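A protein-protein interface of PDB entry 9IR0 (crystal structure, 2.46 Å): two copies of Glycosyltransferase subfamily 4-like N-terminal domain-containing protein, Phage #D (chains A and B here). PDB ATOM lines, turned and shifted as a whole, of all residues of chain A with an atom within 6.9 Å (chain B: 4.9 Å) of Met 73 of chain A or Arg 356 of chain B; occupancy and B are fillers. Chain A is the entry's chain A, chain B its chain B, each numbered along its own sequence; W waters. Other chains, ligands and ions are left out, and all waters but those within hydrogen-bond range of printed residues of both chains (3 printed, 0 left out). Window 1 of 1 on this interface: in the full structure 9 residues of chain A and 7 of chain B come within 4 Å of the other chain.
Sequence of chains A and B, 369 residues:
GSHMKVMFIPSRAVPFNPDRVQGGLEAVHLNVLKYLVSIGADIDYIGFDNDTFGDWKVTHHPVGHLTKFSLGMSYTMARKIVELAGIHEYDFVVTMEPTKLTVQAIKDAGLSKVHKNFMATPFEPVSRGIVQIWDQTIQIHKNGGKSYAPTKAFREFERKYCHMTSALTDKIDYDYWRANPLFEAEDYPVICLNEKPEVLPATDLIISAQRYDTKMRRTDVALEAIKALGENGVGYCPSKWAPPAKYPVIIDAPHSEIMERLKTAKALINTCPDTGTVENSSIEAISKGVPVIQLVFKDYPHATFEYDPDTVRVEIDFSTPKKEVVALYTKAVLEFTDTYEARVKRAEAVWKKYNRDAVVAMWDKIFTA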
ATOM      1  N   ILE A  46       8.584  22.454   8.824  1.00  0.00           N
ATOM      2  CA  ILE A  46       9.031  21.773   7.621  1.00  0.00           C
ATOM      3  C   ILE A  46       9.684  20.457   8.029  1.00  0.00           C
ATOM      4  O   ILE A  46      10.900  20.391   8.209  1.00  0.00           O
ATOM      5  CB  ILE A  46       9.981  22.659   6.789  1.00  0.00           C
ATOM      6  CG1 ILE A  46       9.332  24.022   6.474  1.00  0.00           C
ATOM      7  CG2 ILE A  46      10.437  21.920   5.515  1.00  0.00           C
ATOM      8  CD1 ILE A  46      10.213  24.985   5.710  1.00  0.00           C
ATOM      9  N   PHE A  48       8.672  15.832   8.435  1.00  0.00           N
ATOM     10  CA  PHE A  48       8.637  14.536   7.782  1.00  0.00           C
ATOM     11  C   PHE A  48       7.269  13.888   7.979  1.00  0.00           C
ATOM     12  O   PHE A  48       6.670  14.011   9.044  1.00  0.00           O
ATOM     13  CB  PHE A  48       9.752  13.650   8.360  1.00  0.00           C
ATOM     14  CG  PHE A  48      11.088  14.355   8.435  1.00  0.00           C
ATOM     15  CD1 PHE A  48      11.861  14.535   7.299  1.00  0.00           C
ATOM     16  CD2 PHE A  48      11.551  14.872   9.632  1.00  0.00           C
ATOM     17  CE1 PHE A  48      13.097  15.183   7.370  1.00  0.00           C
ATOM     18  CE2 PHE A  48      12.774  15.534   9.696  1.00  0.00           C
ATOM     19  CZ  PHE A  48      13.535  15.691   8.565  1.00  0.00           C
ATOM     20  N   ASP A  49       6.794  13.179   6.950  1.00  0.00           N
ATOM     21  CA  ASP A  49       5.452  12.619   6.945  1.00  0.00           C
ATOM     22  C   ASP A  49       5.139  11.766   8.175  1.00  0.00           C
ATOM     23  O   ASP A  49       3.986  11.700   8.599  1.00  0.00           O
ATOM     24  CB  ASP A  49       5.230  11.788   5.675  1.00  0.00           C
ATOM     25  CG  ASP A  49       5.211  12.607   4.400  1.00  0.00           C
ATOM     26  OD1 ASP A  49       6.263  13.172   4.043  1.00  0.00           O
ATOM     27  OD2 ASP A  49       4.134  12.706   3.774  1.00  0.00           O
ATOM     28  N   VAL A  63       8.398  16.831   3.905  1.00  0.00           N
ATOM     29  CA  VAL A  63       9.344  16.710   2.804  1.00  0.00           C
ATOM     30  C   VAL A  63       9.679  15.257   2.462  1.00  0.00           C
ATOM     31  O   VAL A  63      10.618  14.997   1.706  1.00  0.00           O
ATOM     32  CB  VAL A  63      10.646  17.502   3.101  1.00  0.00           C
ATOM     33  CG1 VAL A  63      10.333  18.932   3.502  1.00  0.00           C
ATOM     34  CG2 VAL A  63      11.504  16.816   4.156  1.00  0.00           C
ATOM     35  N   GLY A  64       8.911  14.319   3.030  1.00  0.00           N
ATOM     36  CA  GLY A  64       9.094  12.898   2.775  1.00  0.00           C
ATOM     37  C   GLY A  64       9.078  12.055   4.048  1.00  0.00           C
ATOM     38  O   GLY A  64       9.216  12.583   5.148  1.00  0.00           O
ATOM     39  N   HIS A  65       8.908  10.740   3.873  1.00  0.00           N
ATOM     40  CA  HIS A  65       8.988   9.783   4.964  1.00  0.00           C
ATOM     41  C   HIS A  65      10.448   9.579   5.362  1.00  0.00           C
ATOM     42  O   HIS A  65      11.267   9.206   4.527  1.00  0.00           O
ATOM     43  CB  HIS A  65       8.358   8.449   4.545  1.00  0.00           C
ATOM     44  CG  HIS A  65       8.296   7.429   5.642  1.00  0.00           C
ATOM     45  ND1 HIS A  65       9.264   6.446   5.768  1.00  0.00           N
ATOM     46  CD2 HIS A  65       7.404   7.292   6.644  1.00  0.00           C
ATOM     47  CE1 HIS A  65       8.923   5.732   6.829  1.00  0.00           C
ATOM     48  NE2 HIS A  65       7.803   6.207   7.385  1.00  0.00           N
ATOM     49  N   LEU A  66      10.760   9.821   6.642  1.00  0.00           N
ATOM     50  CA  LEU A  66      12.135   9.799   7.118  1.00  0.00           C
ATOM     51  C   LEU A  66      12.534   8.434   7.671  1.00  0.00           C
ATOM     52  O   LEU A  66      11.923   7.941   8.614  1.00  0.00           O
ATOM     53  CB  LEU A  66      12.339  10.852   8.213  1.00  0.00           C
ATOM     54  CG  LEU A  66      13.750  10.925   8.808  1.00  0.00           C
ATOM     55  CD1 LEU A  66      14.769  11.355   7.775  1.00  0.00           C
ATOM     56  CD2 LEU A  66      13.809  11.877   9.969  1.00  0.00           C
ATOM     57  N   THR A  67      13.562   7.840   7.055  1.00  0.00           N
ATOM     58  CA  THR A  67      14.295   6.729   7.638  1.00  0.00           C
ATOM     59  C   THR A  67      15.744   7.191   7.755  1.00  0.00           C
ATOM     60  O   THR A  67      16.271   7.299   8.858  1.00  0.00           O
ATOM     61  CB  THR A  67      14.111   5.446   6.822  1.00  0.00           C
ATOM     62  OG1 THR A  67      12.715   5.226   6.608  1.00  0.00           O
ATOM     63  CG2 THR A  67      14.712   4.232   7.514  1.00  0.00           C
ATOM     64  N   LYS A  68      16.368   7.472   6.605  1.00  0.00           N
ATOM     65  CA  LYS A  68      17.648   8.158   6.560  1.00  0.00           C
ATOM     66  C   LYS A  68      17.459   9.430   5.740  1.00  0.00           C
ATOM     67  O   LYS A  68      16.919   9.378   4.640  1.00  0.00           O
ATOM     68  CB  LYS A  68      18.742   7.264   5.952  1.00  0.00           C
ATOM     69  CG  LYS A  68      20.154   7.819   6.135  1.00  0.00           C
ATOM     70  CD  LYS A  68      21.200   6.713   6.137  1.00  0.00           C
ATOM     71  CE  LYS A  68      22.567   7.160   6.590  1.00  0.00           C
ATOM     72  NZ  LYS A  68      23.474   5.993   6.786  1.00  0.00           N
ATOM     73  N   PHE A  69      17.880  10.573   6.297  1.00  0.00           N
ATOM     74  CA  PHE A  69      17.750  11.852   5.620  1.00  0.00           C
ATOM     75  C   PHE A  69      18.543  11.811   4.318  1.00  0.00           C
ATOM     76  O   PHE A  69      19.710  11.431   4.319  1.00  0.00           O
ATOM     77  CB  PHE A  69      18.247  13.005   6.498  1.00  0.00           C
ATOM     78  CG  PHE A  69      17.906  14.378   5.968  1.00  0.00           C
ATOM     79  CD1 PHE A  69      16.608  14.853   6.022  1.00  0.00           C
ATOM     80  CD2 PHE A  69      18.880  15.188   5.407  1.00  0.00           C
ATOM     81  CE1 PHE A  69      16.290  16.116   5.533  1.00  0.00           C
ATOM     82  CE2 PHE A  69      18.556  16.450   4.909  1.00  0.00           C
ATOM     83  CZ  PHE A  69      17.262  16.905   4.980  1.00  0.00           C
ATOM     84  N   SER A  70      17.889  12.195   3.216  1.00  0.00           N
ATOM     85  CA  SER A  70      18.467  12.083   1.888  1.00  0.00           C
ATOM     86  C   SER A  70      18.649  13.452   1.240  1.00  0.00           C
ATOM     87  O   SER A  70      18.141  14.454   1.736  1.00  0.00           O
ATOM     88  CB  SER A  70      17.590  11.209   0.997  1.00  0.00           C
ATOM     89  OG  SER A  70      16.335  11.827   0.764  1.00  0.00           O
ATOM     90  N   LEU A  71      19.373  13.470   0.115  1.00  0.00           N
ATOM     91  CA  LEU A  71      19.582  14.686  -0.654  1.00  0.00           C
ATOM     92  C   LEU A  71      18.261  15.223  -1.196  1.00  0.00           C
ATOM     93  O   LEU A  71      18.004  16.418  -1.108  1.00  0.00           O
ATOM     94  CB  LEU A  71      20.558  14.441  -1.823  1.00  0.00           C
ATOM     95  CG  LEU A  71      22.048  14.585  -1.510  1.00  0.00           C
ATOM     96  CD1 LEU A  71      22.883  14.358  -2.754  1.00  0.00           C
ATOM     97  CD2 LEU A  71      22.368  15.953  -0.916  1.00  0.00           C
ATOM     98  N   GLY A  72      17.436  14.331  -1.753  1.00  0.00           N
ATOM     99  CA  GLY A  72      16.116  14.695  -2.246  1.00  0.00           C
ATOM    100  C   GLY A  72      15.266  15.417  -1.203  1.00  0.00           C
ATOM    101  O   GLY A  72      14.641  16.433  -1.498  1.00  0.00           O
ATOM    102  N   MET A  73      15.271  14.878   0.021  1.00  0.00           N
ATOM    103  CA  MET A  73      14.566  15.478   1.142  1.00  0.00           C
ATOM    104  C   MET A  73      15.098  16.878   1.448  1.00  0.00           C
ATOM    105  O   MET A  73      14.324  17.793   1.724  1.00  0.00           O
ATOM    106  CB  MET A  73      14.714  14.593   2.385  1.00  0.00           C
ATOM    107  CG  MET A  73      13.673  13.521   2.512  1.00  0.00           C
ATOM    108  SD  MET A  73      14.037  12.432   3.919  1.00  0.00           S
ATOM    109  CE  MET A  73      13.748  10.845   3.184  1.00  0.00           C
ATOM    110  N   SER A  74      16.426  17.032   1.394  1.00  0.00           N
ATOM    111  CA  SER A  74      17.073  18.300   1.685  1.00  0.00           C
ATOM    112  C   SER A  74      16.691  19.381   0.674  1.00  0.00           C
ATOM    113  O   SER A  74      16.414  20.515   1.057  1.00  0.00           O
ATOM    114  CB  SER A  74      18.589  18.129   1.727  1.00  0.00           C
ATOM    115  OG  SER A  74      19.207  19.245   2.340  1.00  0.00           O
ATOM    116  N   TYR A  75      16.669  19.027  -0.616  1.00  0.00           N
ATOM    117  CA  TYR A  75      16.275  19.969  -1.654  1.00  0.00           C
ATOM    118  C   TYR A  75      14.781  20.281  -1.609  1.00  0.00           C
ATOM    119  O   TYR A  75      14.380  21.408  -1.889  1.00  0.00           O
ATOM    120  CB  TYR A  75      16.702  19.480  -3.048  1.00  0.00           C
ATOM    121  CG  TYR A  75      18.136  19.829  -3.360  1.00  0.00           C
ATOM    122  CD1 TYR A  75      19.181  19.051  -2.887  1.00  0.00           C
ATOM    123  CD2 TYR A  75      18.451  20.974  -4.079  1.00  0.00           C
ATOM    124  CE1 TYR A  75      20.506  19.380  -3.157  1.00  0.00           C
ATOM    125  CE2 TYR A  75      19.771  21.315  -4.353  1.00  0.00           C
ATOM    126  CZ  TYR A  75      20.797  20.515  -3.889  1.00  0.00           C
ATOM    127  OH  TYR A  75      22.101  20.856  -4.159  1.00  0.00           O
ATOM    128  N   THR A  76      13.960  19.290  -1.245  1.00  0.00           N
ATOM    129  CA  THR A  76      12.547  19.540  -1.003  1.00  0.00           C
ATOM    130  C   THR A  76      12.392  20.548   0.137  1.00  0.00           C
ATOM    131  O   THR A  76      11.619  21.498   0.037  1.00  0.00           O
ATOM    132  CB  THR A  76      11.789  18.240  -0.704  1.00  0.00           C
ATOM    133  OG1 THR A  76      12.023  17.278  -1.736  1.00  0.00           O
ATOM    134  CG2 THR A  76      10.291  18.475  -0.578  1.00  0.00           C
ATOM    135  N   MET A  77      13.144  20.332   1.220  1.00  0.00           N
ATOM    136  CA  MET A  77      13.114  21.205   2.384  1.00  0.00           C
ATOM    137  C   MET A  77      13.545  22.623   2.012  1.00  0.00           C
ATOM    138  O   MET A  77      12.862  23.585   2.348  1.00  0.00           O
ATOM    139  CB  MET A  77      14.000  20.599   3.500  1.00  0.00           C
ATOM    140  CG  MET A  77      14.364  21.557   4.613  1.00  0.00           C
ATOM    141  SD  MET A  77      15.263  20.736   5.966  1.00  0.00           S
ATOM    142  CE  MET A  77      14.093  19.463   6.426  1.00  0.00           C
ATOM    143  N   ALA A  78      14.673  22.744   1.303  1.00  0.00           N
ATOM    144  CA  ALA A  78      15.184  24.036   0.871  1.00  0.00           C
ATOM    145  C   ALA A  78      14.187  24.772  -0.023  1.00  0.00           C
ATOM    146  O   ALA A  78      14.019  25.979   0.107  1.00  0.00           O
ATOM    147  CB  ALA A  78      16.512  23.863   0.145  1.00  0.00           C
ATOM    148  N   ARG A  79      13.536  24.032  -0.927  1.00  0.00           N
ATOM    149  CA  ARG A  79      12.508  24.586  -1.796  1.00  0.00           C
ATOM    150  C   ARG A  79      11.324  25.108  -0.984  1.00  0.00           C
ATOM    151  O   ARG A  79      10.794  26.176  -1.278  1.00  0.00           O
ATOM    152  CB  ARG A  79      12.052  23.509  -2.805  1.00  0.00           C
ATOM    153  CG  ARG A  79      10.940  23.907  -3.772  1.00  0.00           C
ATOM    154  CD  ARG A  79      11.388  24.931  -4.783  1.00  0.00           C
ATOM    155  NE  ARG A  79      10.268  25.437  -5.571  1.00  0.00           N
ATOM    156  CZ  ARG A  79       9.757  26.656  -5.456  1.00  0.00           C
ATOM    157  NH1 ARG A  79      10.005  27.414  -4.399  1.00  0.00           N
ATOM    158  NH2 ARG A  79       8.959  27.119  -6.414  1.00  0.00           N
ATOM    159  N   LEU A 101      22.666  23.498   2.658  1.00  0.00           N
ATOM    160  CA  LEU A 101      21.572  23.871   1.775  1.00  0.00           C
ATOM    161  C   LEU A 101      20.476  24.649   2.506  1.00  0.00           C
ATOM    162  O   LEU A 101      19.955  25.627   1.973  1.00  0.00           O
ATOM    163  CB  LEU A 101      21.003  22.597   1.143  1.00  0.00           C
ATOM    164  CG  LEU A 101      20.169  22.784  -0.114  1.00  0.00           C
ATOM    165  CD1 LEU A 101      21.036  23.236  -1.282  1.00  0.00           C
ATOM    166  CD2 LEU A 101      19.443  21.511  -0.464  1.00  0.00           C
ATOM    167  N   CYS B 192      13.182  -0.469  -2.059  1.00  0.00           N
ATOM    168  CA  CYS B 192      13.601   0.864  -1.656  1.00  0.00           C
ATOM    169  C   CYS B 192      14.695   0.774  -0.597  1.00  0.00           C
ATOM    170  O   CYS B 192      14.449   0.300   0.511  1.00  0.00           O
ATOM    171  CB  CYS B 192      12.407   1.678  -1.160  1.00  0.00           C
ATOM    172  SG  CYS B 192      12.800   3.396  -0.725  1.00  0.00           S
ATOM    173  N   LEU B 193      15.905   1.214  -0.962  1.00  0.00           N
ATOM    174  CA  LEU B 193      17.035   1.218  -0.050  1.00  0.00           C
ATOM    175  C   LEU B 193      17.209   2.615   0.532  1.00  0.00           C
ATOM    176  O   LEU B 193      17.551   3.546  -0.189  1.00  0.00           O
ATOM    177  CB  LEU B 193      18.311   0.784  -0.787  1.00  0.00           C
ATOM    178  CG  LEU B 193      18.262  -0.603  -1.409  1.00  0.00           C
ATOM    179  CD1 LEU B 193      19.524  -0.901  -2.150  1.00  0.00           C
ATOM    180  CD2 LEU B 193      18.015  -1.672  -0.350  1.00  0.00           C
ATOM    181  N   ASN B 194      16.981   2.746   1.842  1.00  0.00           N
ATOM    182  CA  ASN B 194      17.057   4.036   2.509  1.00  0.00           C
ATOM    183  C   ASN B 194      18.494   4.406   2.863  1.00  0.00           C
ATOM    184  O   ASN B 194      18.879   5.568   2.746  1.00  0.00           O
ATOM    185  CB  ASN B 194      16.168   4.050   3.740  1.00  0.00           C
ATOM    186  CG  ASN B 194      14.708   3.892   3.394  1.00  0.00           C
ATOM    187  OD1 ASN B 194      14.022   2.998   3.890  1.00  0.00           O
ATOM    188  ND2 ASN B 194      14.201   4.755   2.526  1.00  0.00           N
ATOM    189  N   TYR B 354      18.018   1.827  -6.866  1.00  0.00           N
ATOM    190  CA  TYR B 354      16.864   1.786  -5.976  1.00  0.00           C
ATOM    191  C   TYR B 354      17.038   2.521  -4.645  1.00  0.00           C
ATOM    192  O   TYR B 354      16.348   2.225  -3.667  1.00  0.00           O
ATOM    193  CB  TYR B 354      16.506   0.324  -5.680  1.00  0.00           C
ATOM    194  CG  TYR B 354      16.067  -0.459  -6.892  1.00  0.00           C
ATOM    195  CD1 TYR B 354      14.830  -0.232  -7.482  1.00  0.00           C
ATOM    196  CD2 TYR B 354      16.886  -1.429  -7.448  1.00  0.00           C
ATOM    197  CE1 TYR B 354      14.425  -0.948  -8.603  1.00  0.00           C
ATOM    198  CE2 TYR B 354      16.491  -2.154  -8.567  1.00  0.00           C
ATOM    199  CZ  TYR B 354      15.258  -1.912  -9.142  1.00  0.00           C
ATOM    200  OH  TYR B 354      14.883  -2.643 -10.244  1.00  0.00           O
ATOM    201  N   ASN B 355      17.958   3.488  -4.602  1.00  0.00           N
ATOM    202  CA  ASN B 355      18.084   4.359  -3.443  1.00  0.00           C
ATOM    203  C   ASN B 355      16.813   5.198  -3.318  1.00  0.00           C
ATOM    204  O   ASN B 355      16.134   5.472  -4.310  1.00  0.00           O
ATOM    205  CB  ASN B 355      19.344   5.248  -3.514  1.00  0.00           C
ATOM    206  CG  ASN B 355      19.332   6.201  -4.709  1.00  0.00           C
ATOM    207  OD1 ASN B 355      18.716   7.296  -4.690  1.00  0.00           O
ATOM    208  ND2 ASN B 355      20.039   5.801  -5.763  1.00  0.00           N
ATOM    209  N   ARG B 356      16.512   5.593  -2.075  1.00  0.00           N
ATOM    210  CA  ARG B 356      15.261   6.250  -1.731  1.00  0.00           C
ATOM    211  C   ARG B 356      14.921   7.387  -2.690  1.00  0.00           C
ATOM    212  O   ARG B 356      13.789   7.466  -3.160  1.00  0.00           O
ATOM    213  CB  ARG B 356      15.332   6.773  -0.278  1.00  0.00           C
ATOM    214  CG  ARG B 356      14.071   7.489   0.208  1.00  0.00           C
ATOM    215  CD  ARG B 356      14.085   8.961  -0.119  1.00  0.00           C
ATOM    216  NE  ARG B 356      12.798   9.590   0.144  1.00  0.00           N
ATOM    217  CZ  ARG B 356      12.489  10.832  -0.205  1.00  0.00           C
ATOM    218  NH1 ARG B 356      13.347  11.600  -0.855  1.00  0.00           N
ATOM    219  NH2 ARG B 356      11.285  11.311   0.096  1.00  0.00           N
ATOM    220  N   ASP B 357      15.897   8.263  -2.962  1.00  0.00           N
ATOM    221  CA  ASP B 357      15.676   9.410  -3.828  1.00  0.00           C
ATOM    222  C   ASP B 357      15.310   9.011  -5.254  1.00  0.00           C
ATOM    223  O   ASP B 357      14.448   9.646  -5.869  1.00  0.00           O
ATOM    224  CB  ASP B 357      16.906  10.325  -3.819  1.00  0.00           C
ATOM    225  CG  ASP B 357      17.041  11.124  -2.538  1.00  0.00           C
ATOM    226  OD1 ASP B 357      16.080  11.137  -1.744  1.00  0.00           O
ATOM    227  OD2 ASP B 357      18.107  11.740  -2.330  1.00  0.00           O
ATOM    228  N   ALA B 358      15.953   7.947  -5.753  1.00  0.00           N
ATOM    229  CA  ALA B 358      15.637   7.414  -7.069  1.00  0.00           C
ATOM    230  C   ALA B 358      14.235   6.802  -7.098  1.00  0.00           C
ATOM    231  O   ALA B 358      13.508   6.946  -8.084  1.00  0.00           O
ATOM    232  CB  ALA B 358      16.685   6.386  -7.483  1.00  0.00           C
ATOM    233  N   VAL B 359      13.875   6.123  -6.000  1.00  0.00           N
ATOM    234  CA  VAL B 359      12.577   5.480  -5.874  1.00  0.00           C
ATOM    235  C   VAL B 359      11.441   6.500  -5.881  1.00  0.00           C
ATOM    236  O   VAL B 359      10.425   6.283  -6.530  1.00  0.00           O
ATOM    237  CB  VAL B 359      12.527   4.588  -4.609  1.00  0.00           C
ATOM    238  CG1 VAL B 359      11.105   4.172  -4.251  1.00  0.00           C
ATOM    239  CG2 VAL B 359      13.404   3.363  -4.772  1.00  0.00           C
ATOM    240  N   VAL B 360      11.609   7.603  -5.147  1.00  0.00           N
ATOM    241  CA  VAL B 360      10.586   8.634  -5.104  1.00  0.00           C
ATOM    242  C   VAL B 360      10.420   9.246  -6.492  1.00  0.00           C
ATOM    243  O   VAL B 360       9.289   9.464  -6.929  1.00  0.00           O
ATOM    244  CB  VAL B 360      10.866   9.682  -4.006  1.00  0.00           C
ATOM    245  CG1 VAL B 360       9.914  10.870  -4.113  1.00  0.00           C
ATOM    246  CG2 VAL B 360      10.785   9.040  -2.618  1.00  0.00           C
HETATM  247  O   HOH W   1       8.682  10.183   0.780  1.00  0.00           O
HETATM  248  O   HOH W   2      10.093  13.930  -0.746  1.00  0.00           O
HETATM  249  O   HOH W   3      11.246   8.199   2.181  1.00  0.00           O
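The side-chain hydroxyl of Ser 70 of chain A is in hydrogen-bond range of the side-chain carboxylate of Asp 357 of chain B (2.6 Å).
The backbone NH (N) of Leu 71 of chain A is in hydrogen-bond range of the side-chain carboxylate (OD2) of Asp 357 of chain B, at 3.3 Å.
The side-chain carboxylate (OD2) of Asp 357 of chain B sits at hydrogen-bond distance from the backbone NH (N) of Gly 72 of chain A (2.7 Å).
NH1 of Arg 356 of chain B lies within hydrogen-bond range of OG of Ser 70 of chain A, 3.4 Å away.
The side-chain hydroxyl (OG1) of Thr 76 of chain A lies within hydrogen-bond range of the backbone carbonyl oxygen (O) of Gly 72 of chain A, at 2.8 Å.
The side-chain amide oxygen (OD1) of Asn 355 of chain B sits close to the backbone NH (N) of Asp 357 of chain B.
O of Leu 193 of chain B lies within hydrogen-bond range of N of Arg 356 of chain B, 3.0 Å away.
NH1 of Arg 356 of chain B is in salt-bridge range of OD1 of Asp 357 of chain B (2.9 Å).
The backbone NH (N) of Met 73 of chain A lies within hydrogen-bond range of the side-chain hydroxyl (OG) of Ser 70 of chain A (3.3 Å).
The backbone NH (N) of Gly 64 of chain A sits close to the side-chain carboxylate (OD1) of Asp 49 of chain A (3.1 Å).
Among the printed residues, merely in contact across the chains: Met 73 of chain A with Arg 356 of chain B (3.4 Å), Lys 68 of chain A with Asn 194 of chain B (3.6 Å), Thr 67 of chain A with Asn 194 of chain B (3.7 Å) and Gly 64 of chain A with Arg 356 of chain B (3.8 Å).
Of chain B, only Arg 356 (3.4 Å) comes within 4 Å of Met 73 of chain A.
Printed residues of chain B within 4 Å of Leu 71 of chain A: Asp 357.
Of the printed residues of chain B, Thr 67 of chain A touches Asn 194 (3.7 Å).
Of the printed residues of chain B, Gly 72 of chain A touches Asp 357 (2.7 Å).
The nearest printed residue of chain B that does not touch Thr 67 of chain A is Arg 356 of chain B (6.9 Å).
Of the 10 printed residues of chain B, 3 touch a printed residue of chain A.
Among the printed residues, 8 pairs touch across the chains.
Among the printed residues, no Asp or Glu carboxylate lies within 4 Å of a Lys or Arg side-chain nitrogen of the other chain.
No position is printed for both chains.
Water W3 bridges O of His 65 of chain A (2.6 Å) and NE of Arg 356 of chain B (2.9 Å).
Water W2 bridges O of Val 63 of chain A (2.7 Å) and NH2 of Arg 356 of chain B (3.0 Å).
Water W1 lies within hydrogen-bond range of NH2 of Arg 356 of chain B (2.9 Å) and N of His 65 of chain A (3.2 Å).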
